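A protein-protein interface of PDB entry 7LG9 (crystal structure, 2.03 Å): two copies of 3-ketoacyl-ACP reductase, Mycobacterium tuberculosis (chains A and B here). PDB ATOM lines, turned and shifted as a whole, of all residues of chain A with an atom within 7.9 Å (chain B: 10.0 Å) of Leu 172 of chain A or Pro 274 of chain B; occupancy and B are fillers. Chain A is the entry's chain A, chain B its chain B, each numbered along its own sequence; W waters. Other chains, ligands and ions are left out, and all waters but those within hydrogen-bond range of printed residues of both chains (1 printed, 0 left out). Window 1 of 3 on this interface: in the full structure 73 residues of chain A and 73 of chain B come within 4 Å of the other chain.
The backbone NH of Val 271 of chain A lies within hydrogen-bond range of the backbone carbonyl oxygen of Val 260 of chain A. O of Val 260 of chain B is in hydrogen-bond range of N of Val 271 of chain B. The backbone carbonyl oxygen (O) of Pro 273 of chain A sits at hydrogen-bond distance from a ring nitrogen (ND1) of His 275 of chain A, 2.8 Å away.
Among the printed residues, pairs that only touch across the chains: Ala 183 of chain A with Gly 187 of chain B (3.3 Å), Ala 186 of chain A with Ala 186 of chain B (3.4 Å), Ala 182 of chain A with Ala 190 of chain B (3.4 Å), Leu 172 of chain A with Leu 193 of chain B (3.5 Å), His 275 of chain A with Val 271 of chain B (3.6 Å), Ser 272 of chain A with Glu 277 of chain B (3.7 Å), Val 271 of chain A with His 275 of chain B (3.7 Å), Gly 171 of chain A with Ala 190 of chain B (3.7 Å), Leu 172 of chain A with Pro 274 of chain B (3.8 Å), Ser 272 of chain A with Pro 274 of chain B (3.8 Å), Gly 174 of chain A with Leu 193 of chain B (3.8 Å), Val 173 of chain A with Leu 193 of chain B (3.9 Å), Pro 274 of chain A with Leu 172 of chain B (3.9 Å), Pro 274 of chain A with Ser 272 of chain B (3.9 Å), Ala 186 of chain A with Ala 190 of chain B (3.9 Å), Ala 183 of chain A with Ala 190 of chain B (3.98 Å) and Gly 174 of chain A with Ala 190 of chain B (3.99 Å).
Water W1 bridges the backbone carbonyl oxygen (O) of Ala 186 of chain A (3.0 Å) and the backbone carbonyl oxygen (O) of Gly 171 of chain B (3.5 Å).
ND1 of His 275 of chain A sits close to NE2 of His 275 of chain B (3.2 Å). The guanidinium group of Arg 197 of chain B sits close to the backbone carbonyl oxygen of Gly 174 of chain A (3.3 Å). O of His 275 of chain B is in hydrogen-bond range of OG of Ser 272 of chain A, 2.7 Å away. NE of Arg 197 of chain B sits at hydrogen-bond distance from O of Val 173 of chain A (2.8 Å). O of Pro 175 of chain A sits at hydrogen-bond distance from OG of Ser 194 of chain B (2.7 Å). The backbone carbonyl oxygen of Gly 174 of chain A sits close to the side-chain hydroxyl of Ser 194 of chain B, at 3.2 Å. O of His 275 of chain A lies within hydrogen-bond range of N of Ser 272 of chain B (2.8 Å).
Leu 172 of chain A touches just these residues of chain B: Leu 193 (3.5 Å) and Pro 274 (3.8 Å). Of chain A, only Leu 172 (3.8 Å) and Ser 272 (3.8 Å) come within 4 Å of Pro 274 of chain B. No residue of chain B comes within 4 Å of Ala 170 of chain A. Gly 171 of chain A touches just one residue of chain B: Ala 190. Printed residues of chain B within 4 Å of Ala 186 of chain A: Ala 186 and Ala 190. Of the printed residues of chain A, Ala 190 of chain B touches Gly 171 (3.7 Å), Gly 174 (3.99 Å), Ala 182 (3.4 Å), Ala 183 (3.98 Å) and Ala 186 (3.9 Å). Of the printed residues of chain A, Val 271 of chain B touches His 275. Of the printed residues of chain B, Pro 274 of chain A touches Leu 172 and Ser 272. Val 260 of chain A touches none of the printed residues of chain B. The nearest residue of chain A that does not touch Pro 274 of chain B is Pro 274 of chain A (4.1 Å). The nearest printed residue of chain A that does not touch Val 271 of chain B is Pro 274 of chain A (4.1 Å).
Leu 172 of chain A touches Pro 274 of chain B, and with the chains exchanged Pro 274 of chain A touches Leu 172 of chain B. Ala 186 of chain B touches its own counterpart, Ala 186 of chain A. Ser 272 of chain A touches His 275 of chain B, and with the chains exchanged His 275 of chain A touches Ser 272 of chain B. His 275 of chain A touches its own counterpart, His 275 of chain B. Positions printed for both chains: 171, 172, 186, 189, 260, 271, 272, 273, 274 and 275. Of the 24 pairs that touch across the chains among the printed residues, 10 have their exchanged pair printed and touching as well.
Hydrophobic or aromatic side chains of chain B within 4 Å of the printed part of chain A: Leu 172, Ala 186, Ala 190, Leu 193, Val 271, Pro 274 and His 275. Among the printed residues, 24 pairs touch across the chains. Among the printed residues, no Asp or Glu carboxylate lies within 4 Å of a Lys or Arg side-chain nitrogen of the other chain.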
ATOM      1  N   SER A 167      29.389 -18.091  13.003  1.00  0.00           N
ATOM      2  CA  SER A 167      29.849 -16.717  12.864  1.00  0.00           C
ATOM      3  C   SER A 167      31.223 -16.577  13.503  1.00  0.00           C
ATOM      4  O   SER A 167      31.980 -17.550  13.582  1.00  0.00           O
ATOM      5  CB  SER A 167      28.862 -15.733  13.495  1.00  0.00           C
ATOM      6  OG  SER A 167      29.213 -14.391  13.202  1.00  0.00           O
ATOM      7  N   SER A 168      31.548 -15.375  13.968  1.00  0.00           N
ATOM      8  CA  SER A 168      32.840 -15.124  14.587  1.00  0.00           C
ATOM      9  C   SER A 168      32.754 -13.844  15.403  1.00  0.00           C
ATOM     10  O   SER A 168      31.896 -12.990  15.167  1.00  0.00           O
ATOM     11  CB  SER A 168      33.955 -15.024  13.540  1.00  0.00           C
ATOM     12  OG  SER A 168      35.153 -14.518  14.106  1.00  0.00           O
ATOM     13  N   GLU A 169      33.661 -13.730  16.375  1.00  0.00           N
ATOM     14  CA  GLU A 169      33.784 -12.503  17.150  1.00  0.00           C
ATOM     15  C   GLU A 169      34.270 -11.333  16.310  1.00  0.00           C
ATOM     16  O   GLU A 169      34.168 -10.186  16.759  1.00  0.00           O
ATOM     17  CB  GLU A 169      34.725 -12.724  18.337  1.00  0.00           C
ATOM     18  CG  GLU A 169      34.072 -13.440  19.508  1.00  0.00           C
ATOM     19  CD  GLU A 169      35.067 -13.875  20.563  1.00  0.00           C
ATOM     20  OE1 GLU A 169      35.878 -14.781  20.276  1.00  0.00           O
ATOM     21  OE2 GLU A 169      35.041 -13.311  21.677  1.00  0.00           O
ATOM     22  N   ALA A 170      34.795 -11.593  15.110  1.00  0.00           N
ATOM     23  CA  ALA A 170      35.170 -10.505  14.213  1.00  0.00           C
ATOM     24  C   ALA A 170      33.960  -9.675  13.805  1.00  0.00           C
ATOM     25  O   ALA A 170      34.085  -8.466  13.581  1.00  0.00           O
ATOM     26  CB  ALA A 170      35.874 -11.062  12.975  1.00  0.00           C
ATOM     27  N   GLY A 171      32.784 -10.301  13.712  1.00  0.00           N
ATOM     28  CA  GLY A 171      31.579  -9.584  13.330  1.00  0.00           C
ATOM     29  C   GLY A 171      31.127  -8.544  14.333  1.00  0.00           C
ATOM     30  O   GLY A 171      30.341  -7.659  13.980  1.00  0.00           O
ATOM     31  N   LEU A 172      31.604  -8.631  15.571  1.00  0.00           N
ATOM     32  CA  LEU A 172      31.264  -7.665  16.610  1.00  0.00           C
ATOM     33  C   LEU A 172      32.291  -6.555  16.760  1.00  0.00           C
ATOM     34  O   LEU A 172      31.929  -5.444  17.157  1.00  0.00           O
ATOM     35  CB  LEU A 172      31.102  -8.373  17.960  1.00  0.00           C
ATOM     36  CG  LEU A 172      30.067  -9.493  18.070  1.00  0.00           C
ATOM     37  CD1 LEU A 172      30.272 -10.278  19.360  1.00  0.00           C
ATOM     38  CD2 LEU A 172      28.651  -8.938  18.006  1.00  0.00           C
ATOM     39  N   VAL A 173      33.556  -6.826  16.446  1.00  0.00           N
ATOM     40  CA  VAL A 173      34.633  -5.880  16.709  1.00  0.00           C
ATOM     41  C   VAL A 173      35.057  -5.190  15.419  1.00  0.00           C
ATOM     42  O   VAL A 173      35.552  -4.058  15.444  1.00  0.00           O
ATOM     43  CB  VAL A 173      35.830  -6.581  17.382  1.00  0.00           C
ATOM     44  CG1 VAL A 173      35.409  -7.177  18.712  1.00  0.00           C
ATOM     45  CG2 VAL A 173      36.396  -7.661  16.475  1.00  0.00           C
ATOM     46  N   GLY A 174      34.852  -5.859  14.286  1.00  0.00           N
ATOM     47  CA  GLY A 174      35.308  -5.359  13.011  1.00  0.00           C
ATOM     48  C   GLY A 174      36.810  -5.147  12.995  1.00  0.00           C
ATOM     49  O   GLY A 174      37.301  -4.015  13.050  1.00  0.00           O
ATOM     50  N   PRO A 175      37.569  -6.238  12.916  1.00  0.00           N
ATOM     51  CA  PRO A 175      39.030  -6.130  13.000  1.00  0.00           C
ATOM     52  C   PRO A 175      39.615  -5.387  11.808  1.00  0.00           C
ATOM     53  O   PRO A 175      39.024  -5.315  10.730  1.00  0.00           O
ATOM     54  CB  PRO A 175      39.497  -7.592  13.020  1.00  0.00           C
ATOM     55  CG  PRO A 175      38.283  -8.386  13.381  1.00  0.00           C
ATOM     56  CD  PRO A 175      37.124  -7.636  12.819  1.00  0.00           C
ATOM     57  N   ALA A 182      34.602 -10.033   8.734  1.00  0.00           N
ATOM     58  CA  ALA A 182      33.707  -9.506   9.759  1.00  0.00           C
ATOM     59  C   ALA A 182      32.322  -9.213   9.195  1.00  0.00           C
ATOM     60  O   ALA A 182      31.311  -9.431   9.874  1.00  0.00           O
ATOM     61  CB  ALA A 182      34.308  -8.245  10.382  1.00  0.00           C
ATOM     62  N   ALA A 183      32.252  -8.720   7.956  1.00  0.00           N
ATOM     63  CA  ALA A 183      30.955  -8.413   7.362  1.00  0.00           C
ATOM     64  C   ALA A 183      30.157  -9.681   7.086  1.00  0.00           C
ATOM     65  O   ALA A 183      28.951  -9.732   7.352  1.00  0.00           O
ATOM     66  CB  ALA A 183      31.142  -7.607   6.078  1.00  0.00           C
ATOM     67  N   LYS A 185      30.488 -12.603   8.628  1.00  0.00           N
ATOM     68  CA  LYS A 185      30.116 -13.226   9.893  1.00  0.00           C
ATOM     69  C   LYS A 185      28.981 -12.479  10.579  1.00  0.00           C
ATOM     70  O   LYS A 185      28.140 -13.102  11.237  1.00  0.00           O
ATOM     71  CB  LYS A 185      31.332 -13.313  10.816  1.00  0.00           C
ATOM     72  CG  LYS A 185      32.371 -14.327  10.372  1.00  0.00           C
ATOM     73  CD  LYS A 185      31.720 -15.649  10.011  1.00  0.00           C
ATOM     74  CE  LYS A 185      32.736 -16.772   9.948  1.00  0.00           C
ATOM     75  NZ  LYS A 185      32.097 -18.077   9.627  1.00  0.00           N
ATOM     76  N   ALA A 186      28.941 -11.153  10.442  1.00  0.00           N
ATOM     77  CA  ALA A 186      27.822 -10.395  10.989  1.00  0.00           C
ATOM     78  C   ALA A 186      26.542 -10.674  10.212  1.00  0.00           C
ATOM     79  O   ALA A 186      25.455 -10.736  10.796  1.00  0.00           O
ATOM     80  CB  ALA A 186      28.144  -8.901  10.984  1.00  0.00           C
ATOM     81  N   THR A 189      24.957 -14.053  11.306  1.00  0.00           N
ATOM     82  CA  THR A 189      24.150 -13.930  12.517  1.00  0.00           C
ATOM     83  C   THR A 189      22.764 -13.382  12.201  1.00  0.00           C
ATOM     84  O   THR A 189      21.750 -13.913  12.669  1.00  0.00           O
ATOM     85  CB  THR A 189      24.860 -13.032  13.533  1.00  0.00           C
ATOM     86  OG1 THR A 189      26.071 -13.663  13.968  1.00  0.00           O
ATOM     87  CG2 THR A 189      23.967 -12.772  14.739  1.00  0.00           C
ATOM     88  N   CYS A 210      30.258 -18.789  17.799  1.00  0.00           N
ATOM     89  CA  CYS A 210      31.434 -17.974  17.493  1.00  0.00           C
ATOM     90  C   CYS A 210      32.634 -18.686  18.098  1.00  0.00           C
ATOM     91  O   CYS A 210      33.049 -18.375  19.226  1.00  0.00           O
ATOM     92  CB  CYS A 210      31.289 -16.556  18.041  1.00  0.00           C
ATOM     93  SG  CYS A 210      29.852 -15.660  17.415  1.00  0.00           S
ATOM     94  N   VAL A 260      23.077 -16.725  20.306  1.00  0.00           N
ATOM     95  CA  VAL A 260      24.447 -16.602  19.825  1.00  0.00           C
ATOM     96  C   VAL A 260      25.382 -17.028  20.949  1.00  0.00           C
ATOM     97  O   VAL A 260      25.240 -16.567  22.087  1.00  0.00           O
ATOM     98  CB  VAL A 260      24.759 -15.166  19.364  1.00  0.00           C
ATOM     99  CG1 VAL A 260      26.208 -15.054  18.921  1.00  0.00           C
ATOM    100  CG2 VAL A 260      23.818 -14.756  18.242  1.00  0.00           C
ATOM    101  N   ILE A 262      29.537 -17.822  22.135  1.00  0.00           N
ATOM    102  CA  ILE A 262      30.986 -17.809  21.976  1.00  0.00           C
ATOM    103  C   ILE A 262      31.544 -18.978  22.775  1.00  0.00           C
ATOM    104  O   ILE A 262      31.224 -19.133  23.960  1.00  0.00           O
ATOM    105  CB  ILE A 262      31.601 -16.480  22.448  1.00  0.00           C
ATOM    106  CG1 ILE A 262      31.080 -15.312  21.609  1.00  0.00           C
ATOM    107  CG2 ILE A 262      33.117 -16.544  22.390  1.00  0.00           C
ATOM    108  CD1 ILE A 262      31.573 -13.960  22.083  1.00  0.00           C
ATOM    109  N   VAL A 271      25.950 -14.624  24.301  1.00  0.00           N
ATOM    110  CA  VAL A 271      25.975 -13.198  23.997  1.00  0.00           C
ATOM    111  C   VAL A 271      24.571 -12.630  24.129  1.00  0.00           C
ATOM    112  O   VAL A 271      23.589 -13.245  23.694  1.00  0.00           O
ATOM    113  CB  VAL A 271      26.546 -12.957  22.588  1.00  0.00           C
ATOM    114  CG1 VAL A 271      26.678 -11.468  22.309  1.00  0.00           C
ATOM    115  CG2 VAL A 271      27.888 -13.654  22.430  1.00  0.00           C
ATOM    116  N   SER A 272      24.469 -11.453  24.737  1.00  0.00           N
ATOM    117  CA  SER A 272      23.205 -10.745  24.841  1.00  0.00           C
ATOM    118  C   SER A 272      22.997  -9.856  23.623  1.00  0.00           C
ATOM    119  O   SER A 272      23.959  -9.472  22.947  1.00  0.00           O
ATOM    120  CB  SER A 272      23.176  -9.905  26.117  1.00  0.00           C
ATOM    121  OG  SER A 272      24.024  -8.775  26.011  1.00  0.00           O
ATOM    122  N   PRO A 273      21.750  -9.527  23.298  1.00  0.00           N
ATOM    123  CA  PRO A 273      21.493  -8.585  22.206  1.00  0.00           C
ATOM    124  C   PRO A 273      22.099  -7.230  22.517  1.00  0.00           C
ATOM    125  O   PRO A 273      22.320  -6.892  23.691  1.00  0.00           O
ATOM    126  CB  PRO A 273      19.960  -8.512  22.152  1.00  0.00           C
ATOM    127  CG  PRO A 273      19.495  -9.779  22.779  1.00  0.00           C
ATOM    128  CD  PRO A 273      20.505 -10.096  23.842  1.00  0.00           C
ATOM    129  N   PRO A 274      22.388  -6.425  21.497  1.00  0.00           N
ATOM    130  CA  PRO A 274      22.930  -5.087  21.756  1.00  0.00           C
ATOM    131  C   PRO A 274      21.895  -4.197  22.426  1.00  0.00           C
ATOM    132  O   PRO A 274      20.712  -4.216  22.079  1.00  0.00           O
ATOM    133  CB  PRO A 274      23.294  -4.574  20.358  1.00  0.00           C
ATOM    134  CG  PRO A 274      22.372  -5.313  19.446  1.00  0.00           C
ATOM    135  CD  PRO A 274      22.207  -6.679  20.057  1.00  0.00           C
ATOM    136  N   HIS A 275      22.350  -3.423  23.403  1.00  0.00           N
ATOM    137  CA  HIS A 275      21.493  -2.514  24.147  1.00  0.00           C
ATOM    138  C   HIS A 275      21.786  -1.075  23.746  1.00  0.00           C
ATOM    139  O   HIS A 275      22.767  -0.779  23.059  1.00  0.00           O
ATOM    140  CB  HIS A 275      21.685  -2.692  25.656  1.00  0.00           C
ATOM    141  CG  HIS A 275      21.192  -4.005  26.177  1.00  0.00           C
ATOM    142  ND1 HIS A 275      21.821  -5.200  25.901  1.00  0.00           N
ATOM    143  CD2 HIS A 275      20.125  -4.311  26.953  1.00  0.00           C
ATOM    144  CE1 HIS A 275      21.165  -6.185  26.488  1.00  0.00           C
ATOM    145  NE2 HIS A 275      20.132  -5.673  27.133  1.00  0.00           N
ATOM    146  N   GLY B 171      19.129  -5.607  11.010  1.00  0.00           N
ATOM    147  CA  GLY B 171      20.333  -6.378  11.261  1.00  0.00           C
ATOM    148  C   GLY B 171      20.453  -6.875  12.687  1.00  0.00           C
ATOM    149  O   GLY B 171      21.174  -7.847  12.938  1.00  0.00           O
ATOM    150  N   LEU B 172      19.761  -6.235  13.628  1.00  0.00           N
ATOM    151  CA  LEU B 172      19.772  -6.677  15.015  1.00  0.00           C
ATOM    152  C   LEU B 172      18.628  -7.629  15.334  1.00  0.00           C
ATOM    153  O   LEU B 172      18.770  -8.486  16.214  1.00  0.00           O
ATOM    154  CB  LEU B 172      19.691  -5.471  15.955  1.00  0.00           C
ATOM    155  CG  LEU B 172      20.567  -4.259  15.637  1.00  0.00           C
ATOM    156  CD1 LEU B 172      20.284  -3.128  16.614  1.00  0.00           C
ATOM    157  CD2 LEU B 172      22.040  -4.631  15.655  1.00  0.00           C
ATOM    158  N   ALA B 186      23.641  -5.861   8.622  1.00  0.00           N
ATOM    159  CA  ALA B 186      24.547  -6.291   9.681  1.00  0.00           C
ATOM    160  C   ALA B 186      25.993  -6.280   9.204  1.00  0.00           C
ATOM    161  O   ALA B 186      26.887  -5.821   9.925  1.00  0.00           O
ATOM    162  CB  ALA B 186      24.156  -7.682  10.179  1.00  0.00           C
ATOM    163  N   GLY B 187      26.242  -6.782   7.993  1.00  0.00           N
ATOM    164  CA  GLY B 187      27.583  -6.722   7.441  1.00  0.00           C
ATOM    165  C   GLY B 187      28.073  -5.304   7.223  1.00  0.00           C
ATOM    166  O   GLY B 187      29.272  -5.033   7.330  1.00  0.00           O
ATOM    167  N   THR B 189      27.413  -2.741   9.157  1.00  0.00           N
ATOM    168  CA  THR B 189      27.878  -2.265  10.457  1.00  0.00           C
ATOM    169  C   THR B 189      29.294  -2.750  10.741  1.00  0.00           C
ATOM    170  O   THR B 189      30.159  -1.968  11.153  1.00  0.00           O
ATOM    171  CB  THR B 189      26.922  -2.726  11.559  1.00  0.00           C
ATOM    172  OG1 THR B 189      25.618  -2.180  11.324  1.00  0.00           O
ATOM    173  CG2 THR B 189      27.418  -2.268  12.925  1.00  0.00           C
ATOM    174  N   ALA B 190      29.550  -4.042  10.522  1.00  0.00           N
ATOM    175  CA  ALA B 190      30.885  -4.583  10.750  1.00  0.00           C
ATOM    176  C   ALA B 190      31.900  -3.975   9.791  1.00  0.00           C
ATOM    177  O   ALA B 190      33.037  -3.688  10.184  1.00  0.00           O
ATOM    178  CB  ALA B 190      30.865  -6.105  10.616  1.00  0.00           C
ATOM    179  N   LEU B 191      31.509  -3.775   8.529  1.00  0.00           N
ATOM    180  CA  LEU B 191      32.401  -3.124   7.573  1.00  0.00           C
ATOM    181  C   LEU B 191      32.784  -1.725   8.039  1.00  0.00           C
ATOM    182  O   LEU B 191      33.948  -1.322   7.927  1.00  0.00           O
ATOM    183  CB  LEU B 191      31.741  -3.069   6.194  1.00  0.00           C
ATOM    184  CG  LEU B 191      32.343  -2.095   5.177  1.00  0.00           C
ATOM    185  CD1 LEU B 191      33.749  -2.513   4.773  1.00  0.00           C
ATOM    186  CD2 LEU B 191      31.446  -1.954   3.955  1.00  0.00           C
ATOM    187  N   THR B 192      31.818  -0.972   8.570  1.00  0.00           N
ATOM    188  CA  THR B 192      32.110   0.376   9.047  1.00  0.00           C
ATOM    189  C   THR B 192      32.970   0.351  10.305  1.00  0.00           C
ATOM    190  O   THR B 192      33.763   1.273  10.529  1.00  0.00           O
ATOM    191  CB  THR B 192      30.807   1.135   9.304  1.00  0.00           C
ATOM    192  OG1 THR B 192      29.913   0.941   8.200  1.00  0.00           O
ATOM    193  CG2 THR B 192      31.070   2.624   9.475  1.00  0.00           C
ATOM    194  N   LEU B 193      32.828  -0.684  11.135  1.00  0.00           N
ATOM    195  CA  LEU B 193      33.696  -0.815  12.303  1.00  0.00           C
ATOM    196  C   LEU B 193      35.145  -1.032  11.889  1.00  0.00           C
ATOM    197  O   LEU B 193      36.060  -0.452  12.485  1.00  0.00           O
ATOM    198  CB  LEU B 193      33.218  -1.960  13.194  1.00  0.00           C
ATOM    199  CG  LEU B 193      31.845  -1.784  13.843  1.00  0.00           C
ATOM    200  CD1 LEU B 193      31.551  -2.922  14.808  1.00  0.00           C
ATOM    201  CD2 LEU B 193      31.747  -0.438  14.544  1.00  0.00           C
ATOM    202  N   SER B 194      35.375  -1.866  10.870  1.00  0.00           N
ATOM    203  CA  SER B 194      36.732  -2.057  10.368  1.00  0.00           C
ATOM    204  C   SER B 194      37.271  -0.776   9.744  1.00  0.00           C
ATOM    205  O   SER B 194      38.453  -0.449   9.904  1.00  0.00           O
ATOM    206  CB  SER B 194      36.767  -3.201   9.354  1.00  0.00           C
ATOM    207  OG  SER B 194      36.571  -4.453   9.985  1.00  0.00           O
ATOM    208  N   ARG B 197      38.399   1.579  12.559  1.00  0.00           N
ATOM    209  CA  ARG B 197      39.682   1.204  13.143  1.00  0.00           C
ATOM    210  C   ARG B 197      40.828   1.460  12.172  1.00  0.00           C
ATOM    211  O   ARG B 197      41.919   1.871  12.584  1.00  0.00           O
ATOM    212  CB  ARG B 197      39.668  -0.266  13.561  1.00  0.00           C
ATOM    213  CG  ARG B 197      38.664  -0.622  14.639  1.00  0.00           C
ATOM    214  CD  ARG B 197      38.873  -2.058  15.099  1.00  0.00           C
ATOM    215  NE  ARG B 197      37.798  -2.532  15.967  1.00  0.00           N
ATOM    216  CZ  ARG B 197      37.786  -2.389  17.288  1.00  0.00           C
ATOM    217  NH1 ARG B 197      38.791  -1.780  17.901  1.00  0.00           N
ATOM    218  NH2 ARG B 197      36.768  -2.855  17.997  1.00  0.00           N
ATOM    219  N   GLY B 258      33.401   4.971  14.876  1.00  0.00           N
ATOM    220  CA  GLY B 258      32.966   3.615  15.143  1.00  0.00           C
ATOM    221  C   GLY B 258      31.680   3.504  15.927  1.00  0.00           C
ATOM    222  O   GLY B 258      31.442   2.479  16.571  1.00  0.00           O
ATOM    223  N   VAL B 260      27.405   3.570  16.361  1.00  0.00           N
ATOM    224  CA  VAL B 260      26.174   3.198  15.674  1.00  0.00           C
ATOM    225  C   VAL B 260      25.028   3.970  16.309  1.00  0.00           C
ATOM    226  O   VAL B 260      24.829   3.904  17.528  1.00  0.00           O
ATOM    227  CB  VAL B 260      25.918   1.681  15.742  1.00  0.00           C
ATOM    228  CG1 VAL B 260      24.510   1.363  15.269  1.00  0.00           C
ATOM    229  CG2 VAL B 260      26.943   0.936  14.901  1.00  0.00           C
ATOM    230  N   LEU B 270      22.174   6.034  20.778  1.00  0.00           N
ATOM    231  CA  LEU B 270      23.511   5.488  20.589  1.00  0.00           C
ATOM    232  C   LEU B 270      23.532   4.038  21.060  1.00  0.00           C
ATOM    233  O   LEU B 270      23.245   3.755  22.228  1.00  0.00           O
ATOM    234  CB  LEU B 270      24.540   6.322  21.353  1.00  0.00           C
ATOM    235  CG  LEU B 270      25.984   5.820  21.355  1.00  0.00           C
ATOM    236  CD1 LEU B 270      26.545   5.793  19.944  1.00  0.00           C
ATOM    237  CD2 LEU B 270      26.843   6.687  22.262  1.00  0.00           C
ATOM    238  N   VAL B 271      23.869   3.125  20.155  1.00  0.00           N
ATOM    239  CA  VAL B 271      23.861   1.700  20.466  1.00  0.00           C
ATOM    240  C   VAL B 271      25.153   1.334  21.183  1.00  0.00           C
ATOM    241  O   VAL B 271      26.246   1.739  20.770  1.00  0.00           O
ATOM    242  CB  VAL B 271      23.682   0.868  19.186  1.00  0.00           C
ATOM    243  CG1 VAL B 271      23.575  -0.612  19.521  1.00  0.00           C
ATOM    244  CG2 VAL B 271      22.458   1.337  18.419  1.00  0.00           C
ATOM    245  N   SER B 272      25.030   0.567  22.261  1.00  0.00           N
ATOM    246  CA  SER B 272      26.228   0.080  22.923  1.00  0.00           C
ATOM    247  C   SER B 272      26.658  -1.254  22.319  1.00  0.00           C
ATOM    248  O   SER B 272      25.829  -1.986  21.768  1.00  0.00           O
ATOM    249  CB  SER B 272      25.980  -0.092  24.421  1.00  0.00           C
ATOM    250  OG  SER B 272      25.168  -1.224  24.685  1.00  0.00           O
ATOM    251  N   PRO B 273      27.942  -1.593  22.397  1.00  0.00           N
ATOM    252  CA  PRO B 273      28.384  -2.881  21.879  1.00  0.00           C
ATOM    253  C   PRO B 273      27.732  -4.015  22.642  1.00  0.00           C
ATOM    254  O   PRO B 273      27.390  -3.872  23.833  1.00  0.00           O
ATOM    255  CB  PRO B 273      29.902  -2.851  22.098  1.00  0.00           C
ATOM    256  CG  PRO B 273      30.120  -1.820  23.146  1.00  0.00           C
ATOM    257  CD  PRO B 273      29.065  -0.792  22.914  1.00  0.00           C
ATOM    258  N   PRO B 274      27.524  -5.161  21.996  1.00  0.00           N
ATOM    259  CA  PRO B 274      26.911  -6.297  22.694  1.00  0.00           C
ATOM    260  C   PRO B 274      27.801  -6.793  23.823  1.00  0.00           C
ATOM    261  O   PRO B 274      29.026  -6.856  23.694  1.00  0.00           O
ATOM    262  CB  PRO B 274      26.763  -7.354  21.591  1.00  0.00           C
ATOM    263  CG  PRO B 274      26.833  -6.593  20.305  1.00  0.00           C
ATOM    264  CD  PRO B 274      27.754  -5.442  20.570  1.00  0.00           C
ATOM    265  N   HIS B 275      27.172  -7.141  24.939  1.00  0.00           N
ATOM    266  CA  HIS B 275      27.856  -7.696  26.096  1.00  0.00           C
ATOM    267  C   HIS B 275      27.470  -9.158  26.273  1.00  0.00           C
ATOM    268  O   HIS B 275      26.583  -9.683  25.593  1.00  0.00           O
ATOM    269  CB  HIS B 275      27.531  -6.894  27.362  1.00  0.00           C
ATOM    270  CG  HIS B 275      26.077  -6.885  27.720  1.00  0.00           C
ATOM    271  ND1 HIS B 275      25.522  -7.785  28.605  1.00  0.00           N
ATOM    272  CD2 HIS B 275      25.064  -6.084  27.312  1.00  0.00           C
ATOM    273  CE1 HIS B 275      24.229  -7.538  28.727  1.00  0.00           C
ATOM    274  NE2 HIS B 275      23.926  -6.511  27.952  1.00  0.00           N
ATOM    275  N   MET B 276      28.154  -9.816  27.202  1.00  0.00           N
ATOM    276  CA  MET B 276      27.917 -11.223  27.490  1.00  0.00           C
ATOM    277  C   MET B 276      26.804 -11.353  28.520  1.00  0.00           C
ATOM    278  O   MET B 276      26.793 -10.636  29.525  1.00  0.00           O
ATOM    279  CB  MET B 276      29.196 -11.890  27.993  1.00  0.00           C
ATOM    280  CG  MET B 276      30.405 -11.584  27.129  1.00  0.00           C
ATOM    281  SD  MET B 276      30.090 -11.917  25.386  1.00  0.00           S
ATOM    282  CE  MET B 276      31.003 -10.582  24.616  1.00  0.00           C
ATOM    283  N   GLU B 277      25.868 -12.264  28.262  1.00  0.00           N
ATOM    284  CA  GLU B 277      24.720 -12.447  29.142  1.00  0.00           C
ATOM    285  C   GLU B 277      25.008 -13.427  30.274  1.00  0.00           C
ATOM    286  O   GLU B 277      24.547 -13.220  31.402  1.00  0.00           O
ATOM    287  CB  GLU B 277      23.510 -12.917  28.328  1.00  0.00           C
ATOM    288  CG  GLU B 277      22.257 -13.191  29.146  1.00  0.00           C
ATOM    289  CD  GLU B 277      21.012 -13.301  28.287  1.00  0.00           C
ATOM    290  OE1 GLU B 277      20.880 -12.513  27.325  1.00  0.00           O
ATOM    291  OE2 GLU B 277      20.166 -14.176  28.567  1.00  0.00           O
HETATM  292  O   HOH W   1      24.261  -9.428  13.228  1.00  0.00           O
